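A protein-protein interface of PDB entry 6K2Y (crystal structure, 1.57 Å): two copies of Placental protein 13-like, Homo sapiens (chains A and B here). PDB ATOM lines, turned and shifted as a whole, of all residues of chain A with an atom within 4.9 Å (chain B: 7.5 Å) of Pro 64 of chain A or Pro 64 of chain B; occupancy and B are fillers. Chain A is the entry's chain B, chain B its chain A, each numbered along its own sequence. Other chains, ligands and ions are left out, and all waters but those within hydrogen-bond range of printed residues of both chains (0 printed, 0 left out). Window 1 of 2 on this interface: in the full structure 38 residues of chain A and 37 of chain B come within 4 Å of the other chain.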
ATOM      1  N   ARG A  58      12.740 -18.942 -14.347  1.00  0.00           N
ATOM      2  CA  ARG A  58      13.581 -17.879 -13.818  1.00  0.00           C
ATOM      3  C   ARG A  58      13.299 -17.754 -12.326  1.00  0.00           C
ATOM      4  O   ARG A  58      12.141 -17.646 -11.919  1.00  0.00           O
ATOM      5  CB  ARG A  58      13.288 -16.572 -14.543  1.00  0.00           C
ATOM      6  CG  ARG A  58      14.489 -15.702 -14.762  1.00  0.00           C
ATOM      7  CD  ARG A  58      14.453 -14.946 -16.109  1.00  0.00           C
ATOM      8  NE  ARG A  58      13.135 -14.431 -16.465  1.00  0.00           N
ATOM      9  CZ  ARG A  58      12.529 -13.426 -15.836  1.00  0.00           C
ATOM     10  NH1 ARG A  58      13.117 -12.835 -14.803  1.00  0.00           N
ATOM     11  NH2 ARG A  58      11.328 -13.018 -16.230  1.00  0.00           N
ATOM     12  N   LEU A  59      14.336 -17.822 -11.512  1.00  0.00           N
ATOM     13  CA  LEU A  59      14.185 -17.716 -10.069  1.00  0.00           C
ATOM     14  C   LEU A  59      15.027 -16.551  -9.571  1.00  0.00           C
ATOM     15  O   LEU A  59      16.224 -16.477  -9.872  1.00  0.00           O
ATOM     16  CB  LEU A  59      14.621 -19.007  -9.377  1.00  0.00           C
ATOM     17  CG  LEU A  59      14.660 -18.946  -7.849  1.00  0.00           C
ATOM     18  CD1 LEU A  59      13.242 -18.818  -7.295  1.00  0.00           C
ATOM     19  CD2 LEU A  59      15.339 -20.192  -7.316  1.00  0.00           C
ATOM     20  N   HIS A  60      14.404 -15.660  -8.802  1.00  0.00           N
ATOM     21  CA  HIS A  60      15.107 -14.550  -8.173  1.00  0.00           C
ATOM     22  C   HIS A  60      15.607 -14.999  -6.811  1.00  0.00           C
ATOM     23  O   HIS A  60      14.837 -15.515  -5.999  1.00  0.00           O
ATOM     24  CB  HIS A  60      14.196 -13.333  -8.011  1.00  0.00           C
ATOM     25  CG  HIS A  60      13.773 -12.714  -9.303  1.00  0.00           C
ATOM     26  ND1 HIS A  60      14.403 -11.616  -9.847  1.00  0.00           N
ATOM     27  CD2 HIS A  60      12.768 -13.031 -10.155  1.00  0.00           C
ATOM     28  CE1 HIS A  60      13.815 -11.289 -10.984  1.00  0.00           C
ATOM     29  NE2 HIS A  60      12.815 -12.128 -11.192  1.00  0.00           N
ATOM     30  N   GLY A  62      16.791 -13.062  -4.435  1.00  0.00           N
ATOM     31  CA  GLY A  62      16.444 -12.102  -3.414  1.00  0.00           C
ATOM     32  C   GLY A  62      14.943 -11.993  -3.185  1.00  0.00           C
ATOM     33  O   GLY A  62      14.130 -12.662  -3.817  1.00  0.00           O
ATOM     34  N   HIS A  63      14.583 -11.106  -2.253  1.00  0.00           N
ATOM     35  CA  HIS A  63      13.188 -10.827  -1.942  1.00  0.00           C
ATOM     36  C   HIS A  63      12.802  -9.489  -2.538  1.00  0.00           C
ATOM     37  O   HIS A  63      13.433  -8.471  -2.199  1.00  0.00           O
ATOM     38  CB  HIS A  63      12.987 -10.792  -0.439  1.00  0.00           C
ATOM     39  CG  HIS A  63      13.310 -12.080   0.237  1.00  0.00           C
ATOM     40  ND1 HIS A  63      14.521 -12.318   0.849  1.00  0.00           N
ATOM     41  CD2 HIS A  63      12.584 -13.212   0.384  1.00  0.00           C
ATOM     42  CE1 HIS A  63      14.521 -13.538   1.358  1.00  0.00           C
ATOM     43  NE2 HIS A  63      13.356 -14.100   1.090  1.00  0.00           N
ATOM     44  N   PRO A  64      11.789  -9.420  -3.392  1.00  0.00           N
ATOM     45  CA  PRO A  64      11.431  -8.140  -3.996  1.00  0.00           C
ATOM     46  C   PRO A  64      10.791  -7.213  -2.981  1.00  0.00           C
ATOM     47  O   PRO A  64       9.977  -7.624  -2.148  1.00  0.00           O
ATOM     48  CB  PRO A  64      10.448  -8.525  -5.108  1.00  0.00           C
ATOM     49  CG  PRO A  64       9.916  -9.840  -4.693  1.00  0.00           C
ATOM     50  CD  PRO A  64      11.026 -10.535  -3.978  1.00  0.00           C
ATOM     51  N   ALA A  65      11.198  -5.952  -3.048  1.00  0.00           N
ATOM     52  CA  ALA A  65      10.610  -4.882  -2.260  1.00  0.00           C
ATOM     53  C   ALA A  65      10.174  -3.796  -3.226  1.00  0.00           C
ATOM     54  O   ALA A  65      10.936  -3.421  -4.114  1.00  0.00           O
ATOM     55  CB  ALA A  65      11.607  -4.329  -1.243  1.00  0.00           C
ATOM     56  N   ILE A  66       8.944  -3.322  -3.085  1.00  0.00           N
ATOM     57  CA  ILE A  66       8.363  -2.410  -4.061  1.00  0.00           C
ATOM     58  C   ILE A  66       7.910  -1.166  -3.320  1.00  0.00           C
ATOM     59  O   ILE A  66       7.232  -1.269  -2.288  1.00  0.00           O
ATOM     60  CB  ILE A  66       7.194  -3.066  -4.821  1.00  0.00           C
ATOM     61  CG1 ILE A  66       7.709  -4.181  -5.734  1.00  0.00           C
ATOM     62  CG2 ILE A  66       6.473  -2.046  -5.658  1.00  0.00           C
ATOM     63  CD1 ILE A  66       7.542  -5.555  -5.159  1.00  0.00           C
ATOM     64  N   LYS A  80      11.610  -0.437  -7.496  1.00  0.00           N
ATOM     65  CA  LYS A  80      11.768  -1.821  -7.089  1.00  0.00           C
ATOM     66  C   LYS A  80      13.220  -2.109  -6.731  1.00  0.00           C
ATOM     67  O   LYS A  80      14.149  -1.559  -7.331  1.00  0.00           O
ATOM     68  CB  LYS A  80      11.302  -2.767  -8.206  1.00  0.00           C
ATOM     69  CG  LYS A  80      11.331  -4.240  -7.839  1.00  0.00           C
ATOM     70  CD  LYS A  80      10.625  -5.076  -8.897  1.00  0.00           C
ATOM     71  CE  LYS A  80      10.049  -6.356  -8.298  1.00  0.00           C
ATOM     72  NZ  LYS A  80       9.064  -6.986  -9.226  1.00  0.00           N
ATOM     73  N   CYS A  81      13.411  -2.970  -5.736  1.00  0.00           N
ATOM     74  CA  CYS A  81      14.732  -3.489  -5.421  1.00  0.00           C
ATOM     75  C   CYS A  81      14.585  -4.886  -4.837  1.00  0.00           C
ATOM     76  O   CYS A  81      13.472  -5.394  -4.633  1.00  0.00           O
ATOM     77  CB  CYS A  81      15.470  -2.566  -4.452  1.00  0.00           C
ATOM     78  SG  CYS A  81      14.722  -2.500  -2.825  1.00  0.00           S
ATOM     79  N   TYR A  82      15.726  -5.520  -4.573  1.00  0.00           N
ATOM     80  CA  TYR A  82      15.746  -6.850  -3.988  1.00  0.00           C
ATOM     81  C   TYR A  82      16.578  -6.837  -2.724  1.00  0.00           C
ATOM     82  O   TYR A  82      17.691  -6.306  -2.707  1.00  0.00           O
ATOM     83  CB  TYR A  82      16.286  -7.894  -4.973  1.00  0.00           C
ATOM     84  CG  TYR A  82      15.268  -8.254  -6.026  1.00  0.00           C
ATOM     85  CD1 TYR A  82      15.106  -7.461  -7.153  1.00  0.00           C
ATOM     86  CD2 TYR A  82      14.444  -9.374  -5.880  1.00  0.00           C
ATOM     87  CE1 TYR A  82      14.160  -7.766  -8.114  1.00  0.00           C
ATOM     88  CE2 TYR A  82      13.499  -9.688  -6.851  1.00  0.00           C
ATOM     89  CZ  TYR A  82      13.363  -8.881  -7.956  1.00  0.00           C
ATOM     90  OH  TYR A  82      12.430  -9.172  -8.925  1.00  0.00           O
ATOM     91  N   ASP B  36       1.529 -15.604  -1.461  1.00  0.00           N
ATOM     92  CA  ASP B  36       2.525 -14.551  -1.663  1.00  0.00           C
ATOM     93  C   ASP B  36       2.549 -13.685  -0.403  1.00  0.00           C
ATOM     94  O   ASP B  36       2.093 -12.534  -0.418  1.00  0.00           O
ATOM     95  CB  ASP B  36       2.190 -13.731  -2.912  1.00  0.00           C
ATOM     96  CG  ASP B  36       3.127 -12.563  -3.134  1.00  0.00           C
ATOM     97  OD1 ASP B  36       4.212 -12.559  -2.548  1.00  0.00           O
ATOM     98  OD2 ASP B  36       2.763 -11.636  -3.890  1.00  0.00           O
ATOM     99  N   GLN B  38       3.456 -11.125   2.404  1.00  0.00           N
ATOM    100  CA  GLN B  38       4.187  -9.880   2.248  1.00  0.00           C
ATOM    101  C   GLN B  38       3.927  -8.982   3.445  1.00  0.00           C
ATOM    102  O   GLN B  38       3.067  -9.247   4.280  1.00  0.00           O
ATOM    103  CB  GLN B  38       3.814  -9.182   0.945  1.00  0.00           C
ATOM    104  CG  GLN B  38       2.347  -9.035   0.695  1.00  0.00           C
ATOM    105  CD  GLN B  38       2.078  -8.722  -0.768  1.00  0.00           C
ATOM    106  OE1 GLN B  38       2.123  -7.566  -1.177  1.00  0.00           O
ATOM    107  NE2 GLN B  38       1.821  -9.758  -1.564  1.00  0.00           N
ATOM    108  N   LEU B  39       4.726  -7.929   3.529  1.00  0.00           N
ATOM    109  CA  LEU B  39       4.593  -6.882   4.528  1.00  0.00           C
ATOM    110  C   LEU B  39       4.278  -5.594   3.784  1.00  0.00           C
ATOM    111  O   LEU B  39       4.924  -5.291   2.778  1.00  0.00           O
ATOM    112  CB  LEU B  39       5.900  -6.716   5.322  1.00  0.00           C
ATOM    113  CG  LEU B  39       6.005  -5.441   6.173  1.00  0.00           C
ATOM    114  CD1 LEU B  39       5.059  -5.512   7.360  1.00  0.00           C
ATOM    115  CD2 LEU B  39       7.432  -5.227   6.626  1.00  0.00           C
ATOM    116  N   PHE B  57       5.875   0.866   1.311  1.00  0.00           N
ATOM    117  CA  PHE B  57       6.908  -0.154   1.217  1.00  0.00           C
ATOM    118  C   PHE B  57       6.220  -1.507   1.280  1.00  0.00           C
ATOM    119  O   PHE B  57       5.489  -1.788   2.231  1.00  0.00           O
ATOM    120  CB  PHE B  57       7.930   0.015   2.343  1.00  0.00           C
ATOM    121  CG  PHE B  57       8.954  -1.075   2.401  1.00  0.00           C
ATOM    122  CD1 PHE B  57      10.075  -1.024   1.588  1.00  0.00           C
ATOM    123  CD2 PHE B  57       8.800  -2.154   3.275  1.00  0.00           C
ATOM    124  CE1 PHE B  57      11.036  -2.028   1.635  1.00  0.00           C
ATOM    125  CE2 PHE B  57       9.764  -3.175   3.332  1.00  0.00           C
ATOM    126  CZ  PHE B  57      10.889  -3.097   2.514  1.00  0.00           C
ATOM    127  N   ARG B  58       6.424  -2.331   0.256  1.00  0.00           N
ATOM    128  CA  ARG B  58       5.889  -3.681   0.229  1.00  0.00           C
ATOM    129  C   ARG B  58       7.052  -4.647   0.048  1.00  0.00           C
ATOM    130  O   ARG B  58       7.863  -4.476  -0.870  1.00  0.00           O
ATOM    131  CB  ARG B  58       4.865  -3.837  -0.891  1.00  0.00           C
ATOM    132  CG  ARG B  58       3.679  -4.710  -0.541  1.00  0.00           C
ATOM    133  CD  ARG B  58       2.435  -4.343  -1.361  1.00  0.00           C
ATOM    134  NE  ARG B  58       2.765  -3.740  -2.648  1.00  0.00           N
ATOM    135  CZ  ARG B  58       3.094  -4.427  -3.740  1.00  0.00           C
ATOM    136  NH1 ARG B  58       3.145  -5.756  -3.705  1.00  0.00           N
ATOM    137  NH2 ARG B  58       3.373  -3.778  -4.870  1.00  0.00           N
ATOM    138  N   LEU B  59       7.162  -5.621   0.939  1.00  0.00           N
ATOM    139  CA  LEU B  59       8.246  -6.597   0.901  1.00  0.00           C
ATOM    140  C   LEU B  59       7.644  -7.989   0.773  1.00  0.00           C
ATOM    141  O   LEU B  59       6.772  -8.360   1.562  1.00  0.00           O
ATOM    142  CB  LEU B  59       9.112  -6.499   2.160  1.00  0.00           C
ATOM    143  CG  LEU B  59      10.174  -7.585   2.334  1.00  0.00           C
ATOM    144  CD1 LEU B  59      11.227  -7.471   1.223  1.00  0.00           C
ATOM    145  CD2 LEU B  59      10.788  -7.522   3.736  1.00  0.00           C
ATOM    146  N   HIS B  60       8.100  -8.755  -0.219  1.00  0.00           N
ATOM    147  CA  HIS B  60       7.642 -10.130  -0.385  1.00  0.00           C
ATOM    148  C   HIS B  60       8.577 -11.067   0.371  1.00  0.00           C
ATOM    149  O   HIS B  60       9.796 -11.010   0.204  1.00  0.00           O
ATOM    150  CB  HIS B  60       7.608 -10.528  -1.858  1.00  0.00           C
ATOM    151  CG  HIS B  60       6.650  -9.735  -2.685  1.00  0.00           C
ATOM    152  ND1 HIS B  60       5.406 -10.210  -3.033  1.00  0.00           N
ATOM    153  CD2 HIS B  60       6.768  -8.520  -3.272  1.00  0.00           C
ATOM    154  CE1 HIS B  60       4.787  -9.315  -3.781  1.00  0.00           C
ATOM    155  NE2 HIS B  60       5.592  -8.280  -3.943  1.00  0.00           N
ATOM    156  N   PHE B  61       8.011 -11.946   1.190  1.00  0.00           N
ATOM    157  CA  PHE B  61       8.831 -12.836   1.994  1.00  0.00           C
ATOM    158  C   PHE B  61       9.316 -14.065   1.237  1.00  0.00           C
ATOM    159  O   PHE B  61      10.193 -14.760   1.744  1.00  0.00           O
ATOM    160  CB  PHE B  61       8.055 -13.283   3.240  1.00  0.00           C
ATOM    161  CG  PHE B  61       7.795 -12.164   4.209  1.00  0.00           C
ATOM    162  CD1 PHE B  61       8.856 -11.458   4.764  1.00  0.00           C
ATOM    163  CD2 PHE B  61       6.504 -11.794   4.528  1.00  0.00           C
ATOM    164  CE1 PHE B  61       8.627 -10.408   5.645  1.00  0.00           C
ATOM    165  CE2 PHE B  61       6.272 -10.745   5.411  1.00  0.00           C
ATOM    166  CZ  PHE B  61       7.332 -10.056   5.962  1.00  0.00           C
ATOM    167  N   GLY B  62       8.755 -14.362   0.064  1.00  0.00           N
ATOM    168  CA  GLY B  62       9.206 -15.466  -0.752  1.00  0.00           C
ATOM    169  C   GLY B  62      10.098 -15.011  -1.897  1.00  0.00           C
ATOM    170  O   GLY B  62      10.378 -13.829  -2.088  1.00  0.00           O
ATOM    171  N   HIS B  63      10.549 -15.994  -2.676  1.00  0.00           N
ATOM    172  CA  HIS B  63      11.411 -15.741  -3.830  1.00  0.00           C
ATOM    173  C   HIS B  63      10.596 -15.898  -5.101  1.00  0.00           C
ATOM    174  O   HIS B  63      10.109 -17.005  -5.357  1.00  0.00           O
ATOM    175  CB  HIS B  63      12.576 -16.720  -3.846  1.00  0.00           C
ATOM    176  CG  HIS B  63      13.487 -16.582  -2.676  1.00  0.00           C
ATOM    177  ND1 HIS B  63      13.428 -17.414  -1.578  1.00  0.00           N
ATOM    178  CD2 HIS B  63      14.471 -15.688  -2.422  1.00  0.00           C
ATOM    179  CE1 HIS B  63      14.344 -17.045  -0.703  1.00  0.00           C
ATOM    180  NE2 HIS B  63      14.997 -16.007  -1.194  1.00  0.00           N
ATOM    181  N   PRO B  64      10.432 -14.874  -5.936  1.00  0.00           N
ATOM    182  CA  PRO B  64       9.589 -15.040  -7.128  1.00  0.00           C
ATOM    183  C   PRO B  64      10.257 -15.944  -8.152  1.00  0.00           C
ATOM    184  O   PRO B  64      11.449 -15.813  -8.446  1.00  0.00           O
ATOM    185  CB  PRO B  64       9.412 -13.615  -7.656  1.00  0.00           C
ATOM    186  CG  PRO B  64      10.577 -12.849  -7.081  1.00  0.00           C
ATOM    187  CD  PRO B  64      10.930 -13.494  -5.785  1.00  0.00           C
ATOM    188  N   ALA B  65       9.464 -16.870  -8.681  1.00  0.00           N
ATOM    189  CA  ALA B  65       9.857 -17.799  -9.723  1.00  0.00           C
ATOM    190  C   ALA B  65       8.904 -17.588 -10.884  1.00  0.00           C
ATOM    191  O   ALA B  65       7.687 -17.620 -10.694  1.00  0.00           O
ATOM    192  CB  ALA B  65       9.790 -19.245  -9.228  1.00  0.00           C
ATOM    193  N   ILE B  66       9.445 -17.331 -12.071  1.00  0.00           N
ATOM    194  CA  ILE B  66       8.627 -16.922 -13.209  1.00  0.00           C
ATOM    195  C   ILE B  66       8.846 -17.913 -14.339  1.00  0.00           C
ATOM    196  O   ILE B  66       9.988 -18.256 -14.658  1.00  0.00           O
ATOM    197  CB  ILE B  66       8.959 -15.486 -13.649  1.00  0.00           C
ATOM    198  CG1 ILE B  66       8.636 -14.515 -12.511  1.00  0.00           C
ATOM    199  CG2 ILE B  66       8.174 -15.108 -14.877  1.00  0.00           C
ATOM    200  CD1 ILE B  66       9.827 -13.729 -12.020  1.00  0.00           C
ATOM    201  N   LYS B  80       3.629 -17.374 -12.469  1.00  0.00           N
ATOM    202  CA  LYS B  80       4.502 -16.926 -11.396  1.00  0.00           C
ATOM    203  C   LYS B  80       4.100 -17.585 -10.087  1.00  0.00           C
ATOM    204  O   LYS B  80       2.913 -17.802  -9.828  1.00  0.00           O
ATOM    205  CB  LYS B  80       4.438 -15.399 -11.271  1.00  0.00           C
ATOM    206  CG  LYS B  80       5.326 -14.758 -10.219  1.00  0.00           C
ATOM    207  CD  LYS B  80       5.412 -13.254 -10.513  1.00  0.00           C
ATOM    208  CE  LYS B  80       6.278 -12.513  -9.525  1.00  0.00           C
ATOM    209  NZ  LYS B  80       6.493 -11.102  -9.973  1.00  0.00           N
ATOM    210  N   CYS B  81       5.088 -17.909  -9.263  1.00  0.00           N
ATOM    211  CA  CYS B  81       4.814 -18.307  -7.893  1.00  0.00           C
ATOM    212  C   CYS B  81       5.920 -17.768  -7.000  1.00  0.00           C
ATOM    213  O   CYS B  81       6.927 -17.232  -7.473  1.00  0.00           O
ATOM    214  CB  CYS B  81       4.702 -19.827  -7.753  1.00  0.00           C
ATOM    215  SG  CYS B  81       6.216 -20.707  -8.145  1.00  0.00           S
ATOM    216  N   TYR B  82       5.722 -17.897  -5.695  1.00  0.00           N
ATOM    217  CA  TYR B  82       6.724 -17.486  -4.718  1.00  0.00           C
ATOM    218  C   TYR B  82       7.237 -18.712  -3.985  1.00  0.00           C
ATOM    219  O   TYR B  82       6.467 -19.418  -3.324  1.00  0.00           O
ATOM    220  CB  TYR B  82       6.151 -16.451  -3.750  1.00  0.00           C
ATOM    221  CG  TYR B  82       6.076 -15.098  -4.395  1.00  0.00           C
ATOM    222  CD1 TYR B  82       5.018 -14.772  -5.222  1.00  0.00           C
ATOM    223  CD2 TYR B  82       7.093 -14.160  -4.224  1.00  0.00           C
ATOM    224  CE1 TYR B  82       4.947 -13.551  -5.841  1.00  0.00           C
ATOM    225  CE2 TYR B  82       7.028 -12.919  -4.853  1.00  0.00           C
ATOM    226  CZ  TYR B  82       5.947 -12.627  -5.651  1.00  0.00           C
ATOM    227  OH  TYR B  82       5.838 -11.423  -6.294  1.00  0.00           O
ATOM    228  N   TYR B  83       8.535 -18.964  -4.118  1.00  0.00           N
ATOM    229  CA  TYR B  83       9.194 -20.059  -3.426  1.00  0.00           C
ATOM    230  C   TYR B  83       9.428 -19.671  -1.973  1.00  0.00           C
ATOM    231  O   TYR B  83      10.084 -18.665  -1.696  1.00  0.00           O
ATOM    232  CB  TYR B  83      10.512 -20.380  -4.127  1.00  0.00           C
ATOM    233  CG  TYR B  83      11.422 -21.300  -3.357  1.00  0.00           C
ATOM    234  CD1 TYR B  83      10.957 -22.514  -2.855  1.00  0.00           C
ATOM    235  CD2 TYR B  83      12.749 -20.961  -3.136  1.00  0.00           C
ATOM    236  CE1 TYR B  83      11.797 -23.362  -2.153  1.00  0.00           C
ATOM    237  CE2 TYR B  83      13.601 -21.807  -2.431  1.00  0.00           C
ATOM    238  CZ  TYR B  83      13.117 -23.005  -1.941  1.00  0.00           C
ATOM    239  OH  TYR B  83      13.958 -23.844  -1.243  1.00  0.00           O
ATOM    240  N   ILE B 112      18.789  -1.425   1.733  1.00  0.00           N
ATOM    241  CA  ILE B 112      18.348  -1.969   0.454  1.00  0.00           C
ATOM    242  C   ILE B 112      17.941  -0.895  -0.550  1.00  0.00           C
ATOM    243  O   ILE B 112      17.910  -1.189  -1.754  1.00  0.00           O
ATOM    244  CB  ILE B 112      17.201  -2.993   0.624  1.00  0.00           C
ATOM    245  CG1 ILE B 112      15.940  -2.323   1.202  1.00  0.00           C
ATOM    246  CG2 ILE B 112      17.640  -4.177   1.486  1.00  0.00           C
ATOM    247  CD1 ILE B 112      14.708  -3.230   1.139  1.00  0.00           C
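Among the printed residues, pairs that only touch across the chains: Ala 65 of chain A with Arg 58 of chain B (3.1 Å), Arg 58 of chain A with Ala 65 of chain B (3.2 Å), His 63 of chain A with His 60 of chain B (3.3 Å), His 60 of chain A with His 63 of chain B (3.3 Å), Gly 62 of chain A with His 63 of chain B (3.3 Å), His 63 of chain A with Gly 62 of chain B (3.4 Å), Pro 64 of chain A with Pro 64 of chain B (3.5 Å), His 60 of chain A with Ile 66 of chain B (3.5 Å), Ile 66 of chain A with His 60 of chain B (3.6 Å), Pro 64 of chain A with Leu 59 of chain B (3.6 Å), Leu 59 of chain A with Pro 64 of chain B (3.7 Å), Ile 66 of chain A with Phe 57 of chain B (3.7 Å), Ala 65 of chain A with Phe 57 of chain B (3.7 Å), Gly 62 of chain A with Pro 64 of chain B (3.8 Å), Pro 64 of chain A with Gly 62 of chain B (3.9 Å), Leu 59 of chain A with Ala 65 of chain B (3.98 Å) and Arg 58 of chain A with Pro 64 of chain B (3.99 Å).
Of the 11 printed residues of chain A, 9 touch a printed residue of chain B.
Hydrophobic or aromatic side chains of chain A that line the printed part of chain B: Leu 59, His 60, His 63, Pro 64, Ala 65 and Ile 66.
Along chain A the printed residues that touch a printed residue of chain B span positions 58 to 81.
Of the 18 printed residues of chain B, 11 touch a printed residue of chain A.
Printed residues of chain B that touch a printed residue of chain A: Phe 57, Arg 58, Leu 59, His 60, Phe 61, Gly 62, His 63, Pro 64, Ala 65, Ile 66 and Ile 112.
Along chain B the printed residues that touch a printed residue of chain A span positions 57 to 112.
Among the printed residues, 24 pairs touch across the chains.
Printed residues of chain B within 4 Å of Pro 64 of chain A: Leu 59 (3.6 Å), His 60 (2.9 Å), Gly 62 (3.9 Å) and Pro 64 (3.5 Å).
Printed residues of chain A within 4 Å of Phe 57 of chain B: Ala 65 and Ile 66.
Of the printed residues of chain A, Phe 61 of chain B touches His 63 (3.2 Å).
Of the printed residues of chain A, Ala 65 of chain B touches Arg 58 and Leu 59.
Of the printed residues of chain A, Ile 66 of chain B touches Arg 58 (2.7 Å) and His 60 (3.5 Å).
Of the printed residues of chain A, Ile 112 of chain B touches Cys 81 (3.6 Å).
The nearest printed residue of chain B that does not touch Pro 64 of chain A is Arg 58 of chain B (4.002 Å).
The nearest printed residue of chain A that does not touch Pro 64 of chain B is Tyr 82 of chain A (4.3 Å).
The nearest printed residue of chain A that does not touch Ile 66 of chain B is Leu 59 of chain A (4.9 Å).
A ring nitrogen (ND1) of His 60 of chain B sits at hydrogen-bond distance from the side-chain carboxylate (OD1) of Asp 36 of chain B (2.7 Å).
The backbone carbonyl oxygen (O) of His 63 of chain B sits at hydrogen-bond distance from the backbone NH (N) of Tyr 83 of chain B, at 2.8 Å.
The backbone NH of Ala 65 of chain A sits at hydrogen-bond distance from the backbone carbonyl oxygen of Cys 81 of chain A (2.8 Å).
The backbone NH of Leu 39 of chain B sits at hydrogen-bond distance from the backbone carbonyl oxygen of Leu 59 of chain B, 2.9 Å away.
O of Cys 81 of chain B is in hydrogen-bond range of N of Ala 65 of chain B, 2.8 Å away.
The side-chain amide oxygen of Gln 38 of chain B sits close to the guanidinium group of Arg 58 of chain B, at 3.3 Å.
Arg 58 of chain A touches Pro 64 of chain B, but with the chains exchanged Pro 64 of chain A does not touch Arg 58 of chain B (4.002 Å).
Leu 59 of chain A touches Ala 65 of chain B, but with the chains exchanged Ala 65 of chain A does not touch Leu 59 of chain B (4.01 Å).
Gly 62 of chain A touches His 63 of chain B, and with the chains exchanged His 63 of chain A touches Gly 62 of chain B.
Gly 62 of chain A touches Pro 64 of chain B, and with the chains exchanged Pro 64 of chain A touches Gly 62 of chain B.
Of the 24 pairs that touch across the chains among the printed residues, 18 have their exchanged pair printed and touching as well.
The backbone carbonyl oxygen (O) of Phe 61 of chain B sits close to a ring nitrogen (NE2) of His 63 of chain A, at 3.3 Å.
The backbone NH of Ile 66 of chain A sits at hydrogen-bond distance from the backbone carbonyl oxygen of Arg 58 of chain B, at 2.7 Å.
The backbone NH (N) of Ile 66 of chain B sits at hydrogen-bond distance from the backbone carbonyl oxygen (O) of Arg 58 of chain A (2.7 Å).
A ring nitrogen (NE2) of His 63 of chain B sits at hydrogen-bond distance from a ring nitrogen (NE2) of His 63 of chain A (3.4 Å).
The backbone carbonyl oxygen (O) of Ile 112 of chain B is in hydrogen-bond range of the side-chain sulfur (SG) of Cys 81 of chain A (3.6 Å).
O of Pro 64 of chain A sits at hydrogen-bond distance from N of His 60 of chain B (2.9 Å).
The backbone carbonyl oxygen (O) of Pro 64 of chain B lies within hydrogen-bond range of the backbone NH (N) of His 60 of chain A (3.0 Å).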
